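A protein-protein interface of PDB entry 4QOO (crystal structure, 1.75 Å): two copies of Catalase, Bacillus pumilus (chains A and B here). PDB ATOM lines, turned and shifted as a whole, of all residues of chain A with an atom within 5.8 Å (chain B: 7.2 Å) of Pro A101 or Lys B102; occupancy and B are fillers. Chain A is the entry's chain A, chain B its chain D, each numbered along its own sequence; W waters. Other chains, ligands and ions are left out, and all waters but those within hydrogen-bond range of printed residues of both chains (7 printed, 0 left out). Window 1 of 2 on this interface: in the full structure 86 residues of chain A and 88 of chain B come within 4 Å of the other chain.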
ATOM      1  N   GLU A  53     -14.379  -5.702  -9.915  1.00  0.00           N
ATOM      2  CA  GLU A  53     -14.891  -4.327  -9.656  1.00  0.00           C
ATOM      3  C   GLU A  53     -13.912  -3.693  -8.665  1.00  0.00           C
ATOM      4  O   GLU A  53     -13.166  -4.400  -7.930  1.00  0.00           O
ATOM      5  CB  GLU A  53     -16.337  -4.303  -9.176  1.00  0.00           C
ATOM      6  CG  GLU A  53     -16.543  -4.856  -7.770  1.00  0.00           C
ATOM      7  CD  GLU A  53     -18.001  -4.798  -7.307  1.00  0.00           C
ATOM      8  OE1 GLU A  53     -18.935  -4.793  -8.148  1.00  0.00           O
ATOM      9  OE2 GLU A  53     -18.208  -4.919  -6.029  1.00  0.00           O
ATOM     10  N   ALA A  58     -17.390   0.940  -6.151  1.00  0.00           N
ATOM     11  CA  ALA A  58     -17.620   0.084  -7.370  1.00  0.00           C
ATOM     12  C   ALA A  58     -18.662   0.661  -8.309  1.00  0.00           C
ATOM     13  O   ALA A  58     -18.546   0.540  -9.498  1.00  0.00           O
ATOM     14  CB  ALA A  58     -17.983  -1.320  -6.952  1.00  0.00           C
ATOM     15  N   ARG A  59     -19.731   1.253  -7.760  1.00  0.00           N
ATOM     16  CA  ARG A  59     -20.793   1.881  -8.560  1.00  0.00           C
ATOM     17  C   ARG A  59     -20.435   3.332  -8.860  1.00  0.00           C
ATOM     18  O   ARG A  59     -20.198   4.096  -7.941  1.00  0.00           O
ATOM     19  CB  ARG A  59     -22.160   1.857  -7.810  1.00  0.00           C
ATOM     20  CG  ARG A  59     -23.204   2.840  -8.325  1.00  0.00           C
ATOM     21  CD  ARG A  59     -23.688   2.643  -9.730  1.00  0.00           C
ATOM     22  NE  ARG A  59     -24.850   1.793  -9.747  1.00  0.00           N
ATOM     23  CZ  ARG A  59     -25.482   1.397 -10.850  1.00  0.00           C
ATOM     24  NH1 ARG A  59     -25.084   1.759 -12.087  1.00  0.00           N
ATOM     25  NH2 ARG A  59     -26.537   0.641 -10.722  1.00  0.00           N
ATOM     26  N   THR A  97     -20.825   5.960  -5.497  1.00  0.00           N
ATOM     27  CA  THR A  97     -21.061   5.585  -4.138  1.00  0.00           C
ATOM     28  C   THR A  97     -19.862   4.859  -3.563  1.00  0.00           C
ATOM     29  O   THR A  97     -18.787   4.885  -4.175  1.00  0.00           O
ATOM     30  CB  THR A  97     -22.377   4.783  -4.029  1.00  0.00           C
ATOM     31  OG1 THR A  97     -22.253   3.535  -4.682  1.00  0.00           O
ATOM     32  CG2 THR A  97     -23.546   5.564  -4.629  1.00  0.00           C
ATOM     33  N   ILE A  99     -19.960   1.640  -0.759  1.00  0.00           N
ATOM     34  CA  ILE A  99     -19.884   0.349  -0.112  1.00  0.00           C
ATOM     35  C   ILE A  99     -20.445  -0.802  -1.029  1.00  0.00           C
ATOM     36  O   ILE A  99     -19.830  -1.871  -1.105  1.00  0.00           O
ATOM     37  CB  ILE A  99     -20.622   0.338   1.208  1.00  0.00           C
ATOM     38  CG1 ILE A  99     -19.796   1.193   2.225  1.00  0.00           C
ATOM     39  CG2 ILE A  99     -20.816  -1.029   1.719  1.00  0.00           C
ATOM     40  CD1 ILE A  99     -18.388   0.691   2.588  1.00  0.00           C
ATOM     41  N   HIS A 100     -21.600  -0.598  -1.627  1.00  0.00           N
ATOM     42  CA  HIS A 100     -22.222  -1.704  -2.361  1.00  0.00           C
ATOM     43  C   HIS A 100     -21.630  -1.936  -3.736  1.00  0.00           C
ATOM     44  O   HIS A 100     -20.917  -1.075  -4.299  1.00  0.00           O
ATOM     45  CB  HIS A 100     -23.732  -1.542  -2.362  1.00  0.00           C
ATOM     46  CG  HIS A 100     -24.321  -1.662  -0.990  1.00  0.00           C
ATOM     47  ND1 HIS A 100     -24.804  -2.851  -0.466  1.00  0.00           N
ATOM     48  CD2 HIS A 100     -24.440  -0.741  -0.008  1.00  0.00           C
ATOM     49  CE1 HIS A 100     -25.253  -2.634   0.764  1.00  0.00           C
ATOM     50  NE2 HIS A 100     -24.998  -1.369   1.080  1.00  0.00           N
ATOM     51  N   PRO A 101     -21.943  -3.118  -4.340  1.00  0.00           N
ATOM     52  CA  PRO A 101     -21.223  -3.462  -5.586  1.00  0.00           C
ATOM     53  C   PRO A 101     -21.698  -2.676  -6.789  1.00  0.00           C
ATOM     54  O   PRO A 101     -22.608  -1.815  -6.676  1.00  0.00           O
ATOM     55  CB  PRO A 101     -21.489  -4.949  -5.726  1.00  0.00           C
ATOM     56  CG  PRO A 101     -21.745  -5.450  -4.331  1.00  0.00           C
ATOM     57  CD  PRO A 101     -22.556  -4.326  -3.738  1.00  0.00           C
ATOM     58  N   LYS A 102     -21.133  -3.010  -7.964  1.00  0.00           N
ATOM     59  CA  LYS A 102     -21.636  -2.564  -9.260  1.00  0.00           C
ATOM     60  C   LYS A 102     -23.080  -3.003  -9.295  1.00  0.00           C
ATOM     61  O   LYS A 102     -23.423  -4.077  -8.801  1.00  0.00           O
ATOM     62  CB  LYS A 102     -20.868  -3.266 -10.401  1.00  0.00           C
ATOM     63  CG  LYS A 102     -19.501  -2.687 -10.741  1.00  0.00           C
ATOM     64  CD  LYS A 102     -18.930  -3.455 -11.948  1.00  0.00           C
ATOM     65  CE  LYS A 102     -19.649  -3.111 -13.251  1.00  0.00           C
ATOM     66  NZ  LYS A 102     -19.540  -1.643 -13.581  1.00  0.00           N
ATOM     67  N   GLY A 103     -23.930  -2.180  -9.886  1.00  0.00           N
ATOM     68  CA  GLY A 103     -25.277  -2.497 -10.059  1.00  0.00           C
ATOM     69  C   GLY A 103     -26.144  -2.038  -8.892  1.00  0.00           C
ATOM     70  O   GLY A 103     -27.332  -2.032  -9.037  1.00  0.00           O
ATOM     71  N   SER A 104     -25.544  -1.669  -7.762  1.00  0.00           N
ATOM     72  CA  SER A 104     -26.324  -1.236  -6.575  1.00  0.00           C
ATOM     73  C   SER A 104     -26.961   0.111  -6.805  1.00  0.00           C
ATOM     74  O   SER A 104     -26.525   0.934  -7.633  1.00  0.00           O
ATOM     75  CB  SER A 104     -25.408  -1.259  -5.332  1.00  0.00           C
ATOM     76  OG  SER A 104     -24.326  -0.322  -5.420  1.00  0.00           O
ATOM     77  N   LYS A 151     -19.444  -3.210   4.907  1.00  0.00           N
ATOM     78  CA  LYS A 151     -19.815  -4.026   3.736  1.00  0.00           C
ATOM     79  C   LYS A 151     -20.867  -5.042   4.169  1.00  0.00           C
ATOM     80  O   LYS A 151     -20.975  -5.418   5.344  1.00  0.00           O
ATOM     81  CB  LYS A 151     -18.599  -4.778   3.182  1.00  0.00           C
ATOM     82  CG  LYS A 151     -17.626  -3.945   2.347  1.00  0.00           C
ATOM     83  CD  LYS A 151     -17.991  -3.900   0.912  1.00  0.00           C
ATOM     84  CE  LYS A 151     -17.146  -2.968   0.078  1.00  0.00           C
ATOM     85  NZ  LYS A 151     -17.421  -3.256  -1.423  1.00  0.00           N
ATOM     86  N   PRO A 152     -21.551  -5.649   3.174  1.00  0.00           N
ATOM     87  CA  PRO A 152     -22.463  -6.696   3.538  1.00  0.00           C
ATOM     88  C   PRO A 152     -21.764  -7.762   4.383  1.00  0.00           C
ATOM     89  O   PRO A 152     -20.575  -8.094   4.174  1.00  0.00           O
ATOM     90  CB  PRO A 152     -22.939  -7.200   2.179  1.00  0.00           C
ATOM     91  CG  PRO A 152     -22.942  -5.951   1.314  1.00  0.00           C
ATOM     92  CD  PRO A 152     -21.771  -5.138   1.810  1.00  0.00           C
ATOM     93  N   ASN A 157     -24.513 -11.664   3.122  1.00  0.00           N
ATOM     94  CA  ASN A 157     -24.496 -10.699   1.985  1.00  0.00           C
ATOM     95  C   ASN A 157     -25.479  -9.562   2.147  1.00  0.00           C
ATOM     96  O   ASN A 157     -25.881  -8.941   1.159  1.00  0.00           O
ATOM     97  CB  ASN A 157     -24.681 -11.433   0.629  1.00  0.00           C
ATOM     98  CG  ASN A 157     -24.144 -10.640  -0.587  1.00  0.00           C
ATOM     99  OD1 ASN A 157     -24.731 -10.649  -1.714  1.00  0.00           O
ATOM    100  ND2 ASN A 157     -23.094 -10.018  -0.397  1.00  0.00           N
ATOM    101  N   ARG B  50     -11.286  -8.725  -4.513  1.00  0.00           N
ATOM    102  CA  ARG B  50     -12.330  -8.901  -5.540  1.00  0.00           C
ATOM    103  C   ARG B  50     -11.868  -9.739  -6.748  1.00  0.00           C
ATOM    104  O   ARG B  50     -10.743  -9.592  -7.180  1.00  0.00           O
ATOM    105  CB  ARG B  50     -12.821  -7.522  -6.038  1.00  0.00           C
ATOM    106  CG  ARG B  50     -13.410  -6.630  -4.975  1.00  0.00           C
ATOM    107  CD  ARG B  50     -14.697  -7.169  -4.301  1.00  0.00           C
ATOM    108  NE  ARG B  50     -14.999  -6.203  -3.244  1.00  0.00           N
ATOM    109  CZ  ARG B  50     -14.702  -6.358  -1.984  1.00  0.00           C
ATOM    110  NH1 ARG B  50     -14.231  -7.489  -1.483  1.00  0.00           N
ATOM    111  NH2 ARG B  50     -14.853  -5.310  -1.162  1.00  0.00           N
ATOM    112  N   ILE B  51     -12.740 -10.639  -7.200  1.00  0.00           N
ATOM    113  CA  ILE B  51     -12.565 -11.385  -8.443  1.00  0.00           C
ATOM    114  C   ILE B  51     -13.669 -10.936  -9.412  1.00  0.00           C
ATOM    115  O   ILE B  51     -14.650 -10.327  -9.001  1.00  0.00           O
ATOM    116  CB  ILE B  51     -12.553 -12.879  -8.138  1.00  0.00           C
ATOM    117  CG1 ILE B  51     -13.945 -13.373  -7.777  1.00  0.00           C
ATOM    118  CG2 ILE B  51     -11.482 -13.129  -7.026  1.00  0.00           C
ATOM    119  CD1 ILE B  51     -13.992 -14.856  -7.546  1.00  0.00           C
ATOM    120  N   PRO B  52     -13.516 -11.219 -10.719  1.00  0.00           N
ATOM    121  CA  PRO B  52     -14.592 -10.908 -11.658  1.00  0.00           C
ATOM    122  C   PRO B  52     -15.903 -11.546 -11.272  1.00  0.00           C
ATOM    123  O   PRO B  52     -15.896 -12.664 -10.767  1.00  0.00           O
ATOM    124  CB  PRO B  52     -14.082 -11.490 -12.963  1.00  0.00           C
ATOM    125  CG  PRO B  52     -12.610 -11.700 -12.804  1.00  0.00           C
ATOM    126  CD  PRO B  52     -12.416 -12.002 -11.330  1.00  0.00           C
ATOM    127  N   GLU B  53     -17.017 -10.820 -11.456  1.00  0.00           N
ATOM    128  CA  GLU B  53     -18.348 -11.396 -11.196  1.00  0.00           C
ATOM    129  C   GLU B  53     -18.646 -12.277 -12.390  1.00  0.00           C
ATOM    130  O   GLU B  53     -18.016 -12.143 -13.475  1.00  0.00           O
ATOM    131  CB  GLU B  53     -19.435 -10.321 -10.999  1.00  0.00           C
ATOM    132  CG  GLU B  53     -19.760  -9.501 -12.229  1.00  0.00           C
ATOM    133  CD  GLU B  53     -20.789  -8.398 -12.016  1.00  0.00           C
ATOM    134  OE1 GLU B  53     -21.006  -7.933 -10.858  1.00  0.00           O
ATOM    135  OE2 GLU B  53     -21.406  -7.984 -13.058  1.00  0.00           O
ATOM    136  N   ARG B  54     -19.623 -13.136 -12.234  1.00  0.00           N
ATOM    137  CA  ARG B  54     -20.159 -13.887 -13.355  1.00  0.00           C
ATOM    138  C   ARG B  54     -20.602 -12.989 -14.490  1.00  0.00           C
ATOM    139  O   ARG B  54     -21.261 -11.955 -14.270  1.00  0.00           O
ATOM    140  CB  ARG B  54     -21.294 -14.779 -12.948  1.00  0.00           C
ATOM    141  CG  ARG B  54     -20.961 -15.831 -11.901  1.00  0.00           C
ATOM    142  CD  ARG B  54     -22.233 -16.335 -11.243  1.00  0.00           C
ATOM    143  NE  ARG B  54     -21.992 -17.448 -10.292  1.00  0.00           N
ATOM    144  CZ  ARG B  54     -21.406 -17.353  -9.105  1.00  0.00           C
ATOM    145  NH1 ARG B  54     -20.931 -16.200  -8.668  1.00  0.00           N
ATOM    146  NH2 ARG B  54     -21.198 -18.423  -8.361  1.00  0.00           N
ATOM    147  N   HIS B  57     -25.878 -13.753 -14.568  1.00  0.00           N
ATOM    148  CA  HIS B  57     -26.318 -14.269 -13.249  1.00  0.00           C
ATOM    149  C   HIS B  57     -25.371 -13.886 -12.151  1.00  0.00           C
ATOM    150  O   HIS B  57     -25.154 -14.654 -11.170  1.00  0.00           O
ATOM    151  CB  HIS B  57     -26.391 -15.807 -13.288  1.00  0.00           C
ATOM    152  CG  HIS B  57     -27.431 -16.353 -14.230  1.00  0.00           C
ATOM    153  ND1 HIS B  57     -28.574 -16.964 -13.771  1.00  0.00           N
ATOM    154  CD2 HIS B  57     -27.469 -16.457 -15.586  1.00  0.00           C
ATOM    155  CE1 HIS B  57     -29.315 -17.326 -14.797  1.00  0.00           C
ATOM    156  NE2 HIS B  57     -28.653 -17.066 -15.912  1.00  0.00           N
ATOM    157  N   ALA B  58     -24.884 -12.659 -12.251  1.00  0.00           N
ATOM    158  CA  ALA B  58     -23.936 -12.139 -11.250  1.00  0.00           C
ATOM    159  C   ALA B  58     -24.538 -12.016  -9.832  1.00  0.00           C
ATOM    160  O   ALA B  58     -23.840 -12.231  -8.840  1.00  0.00           O
ATOM    161  CB  ALA B  58     -23.332 -10.826 -11.702  1.00  0.00           C
ATOM    162  N   ARG B  59     -25.781 -11.602  -9.760  1.00  0.00           N
ATOM    163  CA  ARG B  59     -26.538 -11.418  -8.484  1.00  0.00           C
ATOM    164  C   ARG B  59     -27.212 -12.721  -8.084  1.00  0.00           C
ATOM    165  O   ARG B  59     -28.003 -13.290  -8.858  1.00  0.00           O
ATOM    166  CB  ARG B  59     -27.620 -10.307  -8.594  1.00  0.00           C
ATOM    167  CG  ARG B  59     -28.726 -10.379  -7.514  1.00  0.00           C
ATOM    168  CD  ARG B  59     -28.246 -10.184  -6.063  1.00  0.00           C
ATOM    169  NE  ARG B  59     -28.300  -8.773  -5.714  1.00  0.00           N
ATOM    170  CZ  ARG B  59     -27.917  -8.244  -4.558  1.00  0.00           C
ATOM    171  NH1 ARG B  59     -27.461  -9.003  -3.554  1.00  0.00           N
ATOM    172  NH2 ARG B  59     -28.065  -6.962  -4.386  1.00  0.00           N
ATOM    173  N   GLY B  60     -26.837 -13.259  -6.932  1.00  0.00           N
ATOM    174  CA  GLY B  60     -27.444 -14.528  -6.509  1.00  0.00           C
ATOM    175  C   GLY B  60     -27.223 -14.901  -5.063  1.00  0.00           C
ATOM    176  O   GLY B  60     -26.541 -14.208  -4.339  1.00  0.00           O
ATOM    177  N   ARG B  94     -27.576 -22.546  -6.124  1.00  0.00           N
ATOM    178  CA  ARG B  94     -27.550 -21.120  -6.249  1.00  0.00           C
ATOM    179  C   ARG B  94     -28.706 -20.659  -7.059  1.00  0.00           C
ATOM    180  O   ARG B  94     -28.929 -21.122  -8.220  1.00  0.00           O
ATOM    181  CB  ARG B  94     -26.181 -20.630  -6.818  1.00  0.00           C
ATOM    182  CG  ARG B  94     -25.952 -19.117  -6.840  1.00  0.00           C
ATOM    183  CD  ARG B  94     -24.549 -18.734  -7.204  1.00  0.00           C
ATOM    184  NE  ARG B  94     -24.324 -17.296  -7.307  1.00  0.00           N
ATOM    185  CZ  ARG B  94     -24.619 -16.549  -8.373  1.00  0.00           C
ATOM    186  NH1 ARG B  94     -25.230 -17.054  -9.392  1.00  0.00           N
ATOM    187  NH2 ARG B  94     -24.343 -15.271  -8.379  1.00  0.00           N
ATOM    188  N   THR B  97     -30.647 -13.731 -10.417  1.00  0.00           N
ATOM    189  CA  THR B  97     -31.160 -13.023 -11.566  1.00  0.00           C
ATOM    190  C   THR B  97     -30.183 -13.246 -12.741  1.00  0.00           C
ATOM    191  O   THR B  97     -29.310 -14.123 -12.660  1.00  0.00           O
ATOM    192  CB  THR B  97     -31.411 -11.521 -11.279  1.00  0.00           C
ATOM    193  OG1 THR B  97     -30.193 -10.858 -10.982  1.00  0.00           O
ATOM    194  CG2 THR B  97     -32.380 -11.343 -10.117  1.00  0.00           C
ATOM    195  N   ILE B  99     -29.249 -10.395 -15.789  1.00  0.00           N
ATOM    196  CA  ILE B  99     -28.588  -9.425 -16.628  1.00  0.00           C
ATOM    197  C   ILE B  99     -27.723  -8.472 -15.804  1.00  0.00           C
ATOM    198  O   ILE B  99     -26.595  -8.123 -16.195  1.00  0.00           O
ATOM    199  CB  ILE B  99     -29.596  -8.704 -17.512  1.00  0.00           C
ATOM    200  CG1 ILE B  99     -30.120  -9.682 -18.600  1.00  0.00           C
ATOM    201  CG2 ILE B  99     -29.007  -7.471 -18.160  1.00  0.00           C
ATOM    202  CD1 ILE B  99     -29.107 -10.242 -19.613  1.00  0.00           C
ATOM    203  N   HIS B 100     -28.253  -7.927 -14.709  1.00  0.00           N
ATOM    204  CA  HIS B 100     -27.538  -6.809 -14.045  1.00  0.00           C
ATOM    205  C   HIS B 100     -26.429  -7.299 -13.130  1.00  0.00           C
ATOM    206  O   HIS B 100     -26.366  -8.493 -12.761  1.00  0.00           O
ATOM    207  CB  HIS B 100     -28.538  -5.858 -13.349  1.00  0.00           C
ATOM    208  CG  HIS B 100     -29.381  -5.101 -14.307  1.00  0.00           C
ATOM    209  ND1 HIS B 100     -29.077  -3.836 -14.772  1.00  0.00           N
ATOM    210  CD2 HIS B 100     -30.500  -5.473 -14.955  1.00  0.00           C
ATOM    211  CE1 HIS B 100     -29.991  -3.468 -15.663  1.00  0.00           C
ATOM    212  NE2 HIS B 100     -30.858  -4.442 -15.778  1.00  0.00           N
ATOM    213  N   PRO B 101     -25.542  -6.392 -12.718  1.00  0.00           N
ATOM    214  CA  PRO B 101     -24.380  -6.850 -11.898  1.00  0.00           C
ATOM    215  C   PRO B 101     -24.673  -7.309 -10.492  1.00  0.00           C
ATOM    216  O   PRO B 101     -25.829  -7.260 -10.050  1.00  0.00           O
ATOM    217  CB  PRO B 101     -23.424  -5.624 -11.938  1.00  0.00           C
ATOM    218  CG  PRO B 101     -23.862  -4.875 -13.160  1.00  0.00           C
ATOM    219  CD  PRO B 101     -25.343  -4.996 -13.171  1.00  0.00           C
ATOM    220  N   LYS B 102     -23.620  -7.710  -9.801  1.00  0.00           N
ATOM    221  CA  LYS B 102     -23.676  -8.258  -8.429  1.00  0.00           C
ATOM    222  C   LYS B 102     -24.585  -7.593  -7.442  1.00  0.00           C
ATOM    223  O   LYS B 102     -25.218  -8.291  -6.636  1.00  0.00           O
ATOM    224  CB  LYS B 102     -22.282  -8.247  -7.811  1.00  0.00           C
ATOM    225  CG  LYS B 102     -21.642  -9.584  -7.941  1.00  0.00           C
ATOM    226  CD  LYS B 102     -20.291  -9.626  -7.229  1.00  0.00           C
ATOM    227  CE  LYS B 102     -20.451  -9.643  -5.713  1.00  0.00           C
ATOM    228  NZ  LYS B 102     -21.241 -10.818  -5.188  1.00  0.00           N
ATOM    229  N   GLY B 103     -24.606  -6.267  -7.403  1.00  0.00           N
ATOM    230  CA  GLY B 103     -25.369  -5.573  -6.320  1.00  0.00           C
ATOM    231  C   GLY B 103     -26.726  -5.028  -6.754  1.00  0.00           C
ATOM    232  O   GLY B 103     -27.400  -4.262  -6.049  1.00  0.00           O
ATOM    233  N   SER B 104     -27.174  -5.520  -7.891  1.00  0.00           N
ATOM    234  CA  SER B 104     -28.409  -5.092  -8.534  1.00  0.00           C
ATOM    235  C   SER B 104     -29.676  -5.625  -7.833  1.00  0.00           C
ATOM    236  O   SER B 104     -29.640  -6.637  -7.066  1.00  0.00           O
ATOM    237  CB  SER B 104     -28.417  -5.480 -10.006  1.00  0.00           C
ATOM    238  OG  SER B 104     -28.386  -6.891 -10.192  1.00  0.00           O
ATOM    239  N   PRO B 105     -30.787  -4.934  -8.038  1.00  0.00           N
ATOM    240  CA  PRO B 105     -31.984  -5.358  -7.272  1.00  0.00           C
ATOM    241  C   PRO B 105     -32.506  -6.722  -7.685  1.00  0.00           C
ATOM    242  O   PRO B 105     -32.446  -7.110  -8.872  1.00  0.00           O
ATOM    243  CB  PRO B 105     -33.012  -4.236  -7.545  1.00  0.00           C
ATOM    244  CG  PRO B 105     -32.153  -3.037  -7.853  1.00  0.00           C
ATOM    245  CD  PRO B 105     -30.993  -3.621  -8.666  1.00  0.00           C
ATOM    246  N   GLU B 106     -33.165  -7.411  -6.741  1.00  0.00           N
ATOM    247  CA  GLU B 106     -33.769  -8.701  -7.050  1.00  0.00           C
ATOM    248  C   GLU B 106     -35.294  -8.570  -7.440  1.00  0.00           C
ATOM    249  O   GLU B 106     -36.003  -9.599  -7.549  1.00  0.00           O
ATOM    250  CB  GLU B 106     -33.566  -9.667  -5.887  1.00  0.00           C
ATOM    251  CG  GLU B 106     -32.131 -10.164  -5.837  1.00  0.00           C
ATOM    252  CD  GLU B 106     -31.794 -10.895  -4.554  1.00  0.00           C
ATOM    253  OE1 GLU B 106     -32.290 -10.490  -3.455  1.00  0.00           O
ATOM    254  OE2 GLU B 106     -31.011 -11.889  -4.624  1.00  0.00           O
ATOM    255  N   PHE B 240     -33.389  -3.769  -1.943  1.00  0.00           N
ATOM    256  CA  PHE B 240     -32.859  -4.233  -3.238  1.00  0.00           C
ATOM    257  C   PHE B 240     -32.279  -5.656  -3.154  1.00  0.00           C
ATOM    258  O   PHE B 240     -31.715  -6.154  -4.151  1.00  0.00           O
ATOM    259  CB  PHE B 240     -31.813  -3.240  -3.848  1.00  0.00           C
ATOM    260  CG  PHE B 240     -30.594  -3.062  -3.031  1.00  0.00           C
ATOM    261  CD1 PHE B 240     -30.605  -2.208  -1.958  1.00  0.00           C
ATOM    262  CD2 PHE B 240     -29.413  -3.693  -3.358  1.00  0.00           C
ATOM    263  CE1 PHE B 240     -29.499  -2.032  -1.142  1.00  0.00           C
ATOM    264  CE2 PHE B 240     -28.273  -3.468  -2.563  1.00  0.00           C
ATOM    265  CZ  PHE B 240     -28.324  -2.640  -1.457  1.00  0.00           C
ATOM    266  N   PHE B 307     -20.101 -16.330   2.354  1.00  0.00           N
ATOM    267  CA  PHE B 307     -20.781 -16.078   1.093  1.00  0.00           C
ATOM    268  C   PHE B 307     -19.760 -16.035  -0.053  1.00  0.00           C
ATOM    269  O   PHE B 307     -19.967 -16.661  -1.110  1.00  0.00           O
ATOM    270  CB  PHE B 307     -21.517 -14.733   1.169  1.00  0.00           C
ATOM    271  CG  PHE B 307     -22.327 -14.413  -0.104  1.00  0.00           C
ATOM    272  CD1 PHE B 307     -23.650 -14.881  -0.274  1.00  0.00           C
ATOM    273  CD2 PHE B 307     -21.773 -13.658  -1.116  1.00  0.00           C
ATOM    274  CE1 PHE B 307     -24.346 -14.629  -1.432  1.00  0.00           C
ATOM    275  CE2 PHE B 307     -22.505 -13.359  -2.263  1.00  0.00           C
ATOM    276  CZ  PHE B 307     -23.781 -13.877  -2.422  1.00  0.00           C
ATOM    277  N   PHE B 308     -18.653 -15.310   0.126  1.00  0.00           N
ATOM    278  CA  PHE B 308     -17.614 -15.328  -0.993  1.00  0.00           C
ATOM    279  C   PHE B 308     -17.081 -16.710  -1.293  1.00  0.00           C
ATOM    280  O   PHE B 308     -17.039 -17.139  -2.474  1.00  0.00           O
ATOM    281  CB  PHE B 308     -16.469 -14.444  -0.675  1.00  0.00           C
ATOM    282  CG  PHE B 308     -15.415 -14.415  -1.748  1.00  0.00           C
ATOM    283  CD1 PHE B 308     -15.541 -13.546  -2.811  1.00  0.00           C
ATOM    284  CD2 PHE B 308     -14.325 -15.241  -1.674  1.00  0.00           C
ATOM    285  CE1 PHE B 308     -14.548 -13.470  -3.836  1.00  0.00           C
ATOM    286  CE2 PHE B 308     -13.315 -15.157  -2.614  1.00  0.00           C
ATOM    287  CZ  PHE B 308     -13.439 -14.282  -3.723  1.00  0.00           C
ATOM    288  N   GLU B 312     -20.154 -17.184  -3.943  1.00  0.00           N
ATOM    289  CA  GLU B 312     -19.526 -16.422  -5.041  1.00  0.00           C
ATOM    290  C   GLU B 312     -18.607 -17.260  -5.894  1.00  0.00           C
ATOM    291  O   GLU B 312     -18.598 -17.110  -7.157  1.00  0.00           O
ATOM    292  CB  GLU B 312     -18.811 -15.159  -4.514  1.00  0.00           C
ATOM    293  CG  GLU B 312     -18.306 -14.308  -5.723  1.00  0.00           C
ATOM    294  CD  GLU B 312     -19.426 -13.667  -6.594  1.00  0.00           C
ATOM    295  OE1 GLU B 312     -19.127 -13.260  -7.736  1.00  0.00           O
ATOM    296  OE2 GLU B 312     -20.554 -13.454  -6.121  1.00  0.00           O
HETATM  297  O   HOH W   1     -24.115  -9.549  -4.737  1.00  0.00           O
HETATM  298  O   HOH W   2     -26.869  -7.790  -1.159  1.00  0.00           O
HETATM  299  O   HOH W   3     -18.237  -6.047  -1.988  1.00  0.00           O
HETATM  300  O   HOH W   4     -18.691  -6.910  -9.685  1.00  0.00           O
HETATM  301  O   HOH W   5     -15.935  -8.011  -8.985  1.00  0.00           O
HETATM  302  O   HOH W   6     -16.547  -3.853  -4.293  1.00  0.00           O
HETATM  303  O   HOH W   7     -27.144 -11.888  -3.137  1.00  0.00           O
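N of Gly B103 is in hydrogen-bond range of O of Lys A102, 2.9 Å away.
The guanidinium group (NH2) of Arg B50 lies close to the side-chain amino group (NZ) of Lys A151.
The guanidinium group (NH2) of Arg B59 sits at hydrogen-bond distance from the backbone carbonyl oxygen (O) of Gly B103, at 3.2 Å.
NZ of Lys B102 lies within salt-bridge range of OE2 of Glu B312 (2.9 Å).
The guanidinium group (NE) of Arg B59 lies within hydrogen-bond range of the backbone carbonyl oxygen (O) of Lys B102 (3.3 Å).
OE1 of Glu A53 is in hydrogen-bond range of N of Lys A102, at 2.8 Å.
The side-chain amino group of Lys A151 lies within hydrogen-bond range of the backbone carbonyl oxygen of Ile A99, 2.8 Å away.
O of Phe B307 lies within hydrogen-bond range of N of Glu B312, 2.9 Å away.
Printed residues of chain B within 4 Å of Pro A101: Lys B102 and Gly B103.
Of the printed residues of chain A, Lys B102 touches Pro A101 and Lys A102.
Of the printed residues of chain B, Glu A53 touches Arg B50.
Of the printed residues of chain B, His A100 touches Phe B240 (3.7 Å).
Ala A58 touches none of the printed residues of chain B.
Water W1 lies within hydrogen-bond range of the backbone carbonyl oxygen of Lys B102 (2.5 Å) and the side-chain amide oxygen of Asn A157 (3.3 Å).
Water W4 lies within hydrogen-bond range of the side-chain carboxylate of Glu A53 (2.6 Å) and the side-chain carboxylate of Glu B53 (2.8 Å).
Water W6 lies within hydrogen-bond range of the side-chain carboxylate of Glu A53, the guanidinium group of Arg B50 and the side-chain amino group of Lys A151.
Water W7 lies within hydrogen-bond range of the backbone carbonyl oxygen (O) of Gly B60 (2.7 Å), the guanidinium group (NH1) of Arg B59 (2.9 Å) and the side-chain amide oxygen (OD1) of Asn A157 (3.1 Å).
Water W2 lies within hydrogen-bond range of the guanidinium group of Arg B59 (2.7 Å) and the backbone carbonyl oxygen of Asn A157 (2.8 Å).
Water W3 lies within hydrogen-bond range of NZ of Lys A151 and NE of Arg B50.
Pro A101 touches Lys B102, and with the chains exchanged Lys A102 touches Pro B101.
Pro A101 touches Gly B103, and with the chains exchanged Gly A103 touches Pro B101.
Lys A102 touches its own counterpart, Lys B102.
Gly B103 touches its own counterpart, Gly A103.
10 positions are printed for both chains.
Of the 14 pairs that touch across the chains among the printed residues, 8 have their exchanged pair printed and touching as well.
Hydrophobic or aromatic side chains of chain A that line the printed part of chain B: His A100 and Pro A101.
Of the 23 printed residues of chain B, 8 touch a printed residue of chain A.
Printed residues of chain B that touch a printed residue of chain A: Arg B50, Arg B59, Pro B101, Lys B102, Gly B103, Ser B104, Phe B240 and Phe B307.
Hydrophobic or aromatic side chains of chain B within 4 Å of the printed part of chain A: Pro B101, Phe B240 and Phe B307.
Among the printed residues, 14 pairs touch across the chains.
Among the printed residues, no Asp or Glu carboxylate lies within 4 Å of a Lys or Arg side-chain nitrogen of the other chain.
CB of Arg B50 touches O of Glu A53, at 3.7 Å.
Phe B240 touches His A100 (CZ to ND1, 3.7 Å).
Pro A101 touches Lys B102 (CB to CB, 3.98 Å).
Pro A101 touches Gly B103 (CB to N, 3.8 Å).
O of Lys A102 touches CB of Pro B101 (3.5 Å).
Pro B101 touches Gly A103 (CD to CA, 3.99 Å).
Gly A103 touches Ser B104 (O to CA, 3.3 Å).
Gly B103 touches Ser A104.
Asn A157 touches Arg B59.
OD1 of Asn A157 touches CZ of Phe B307 (3.4 Å).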
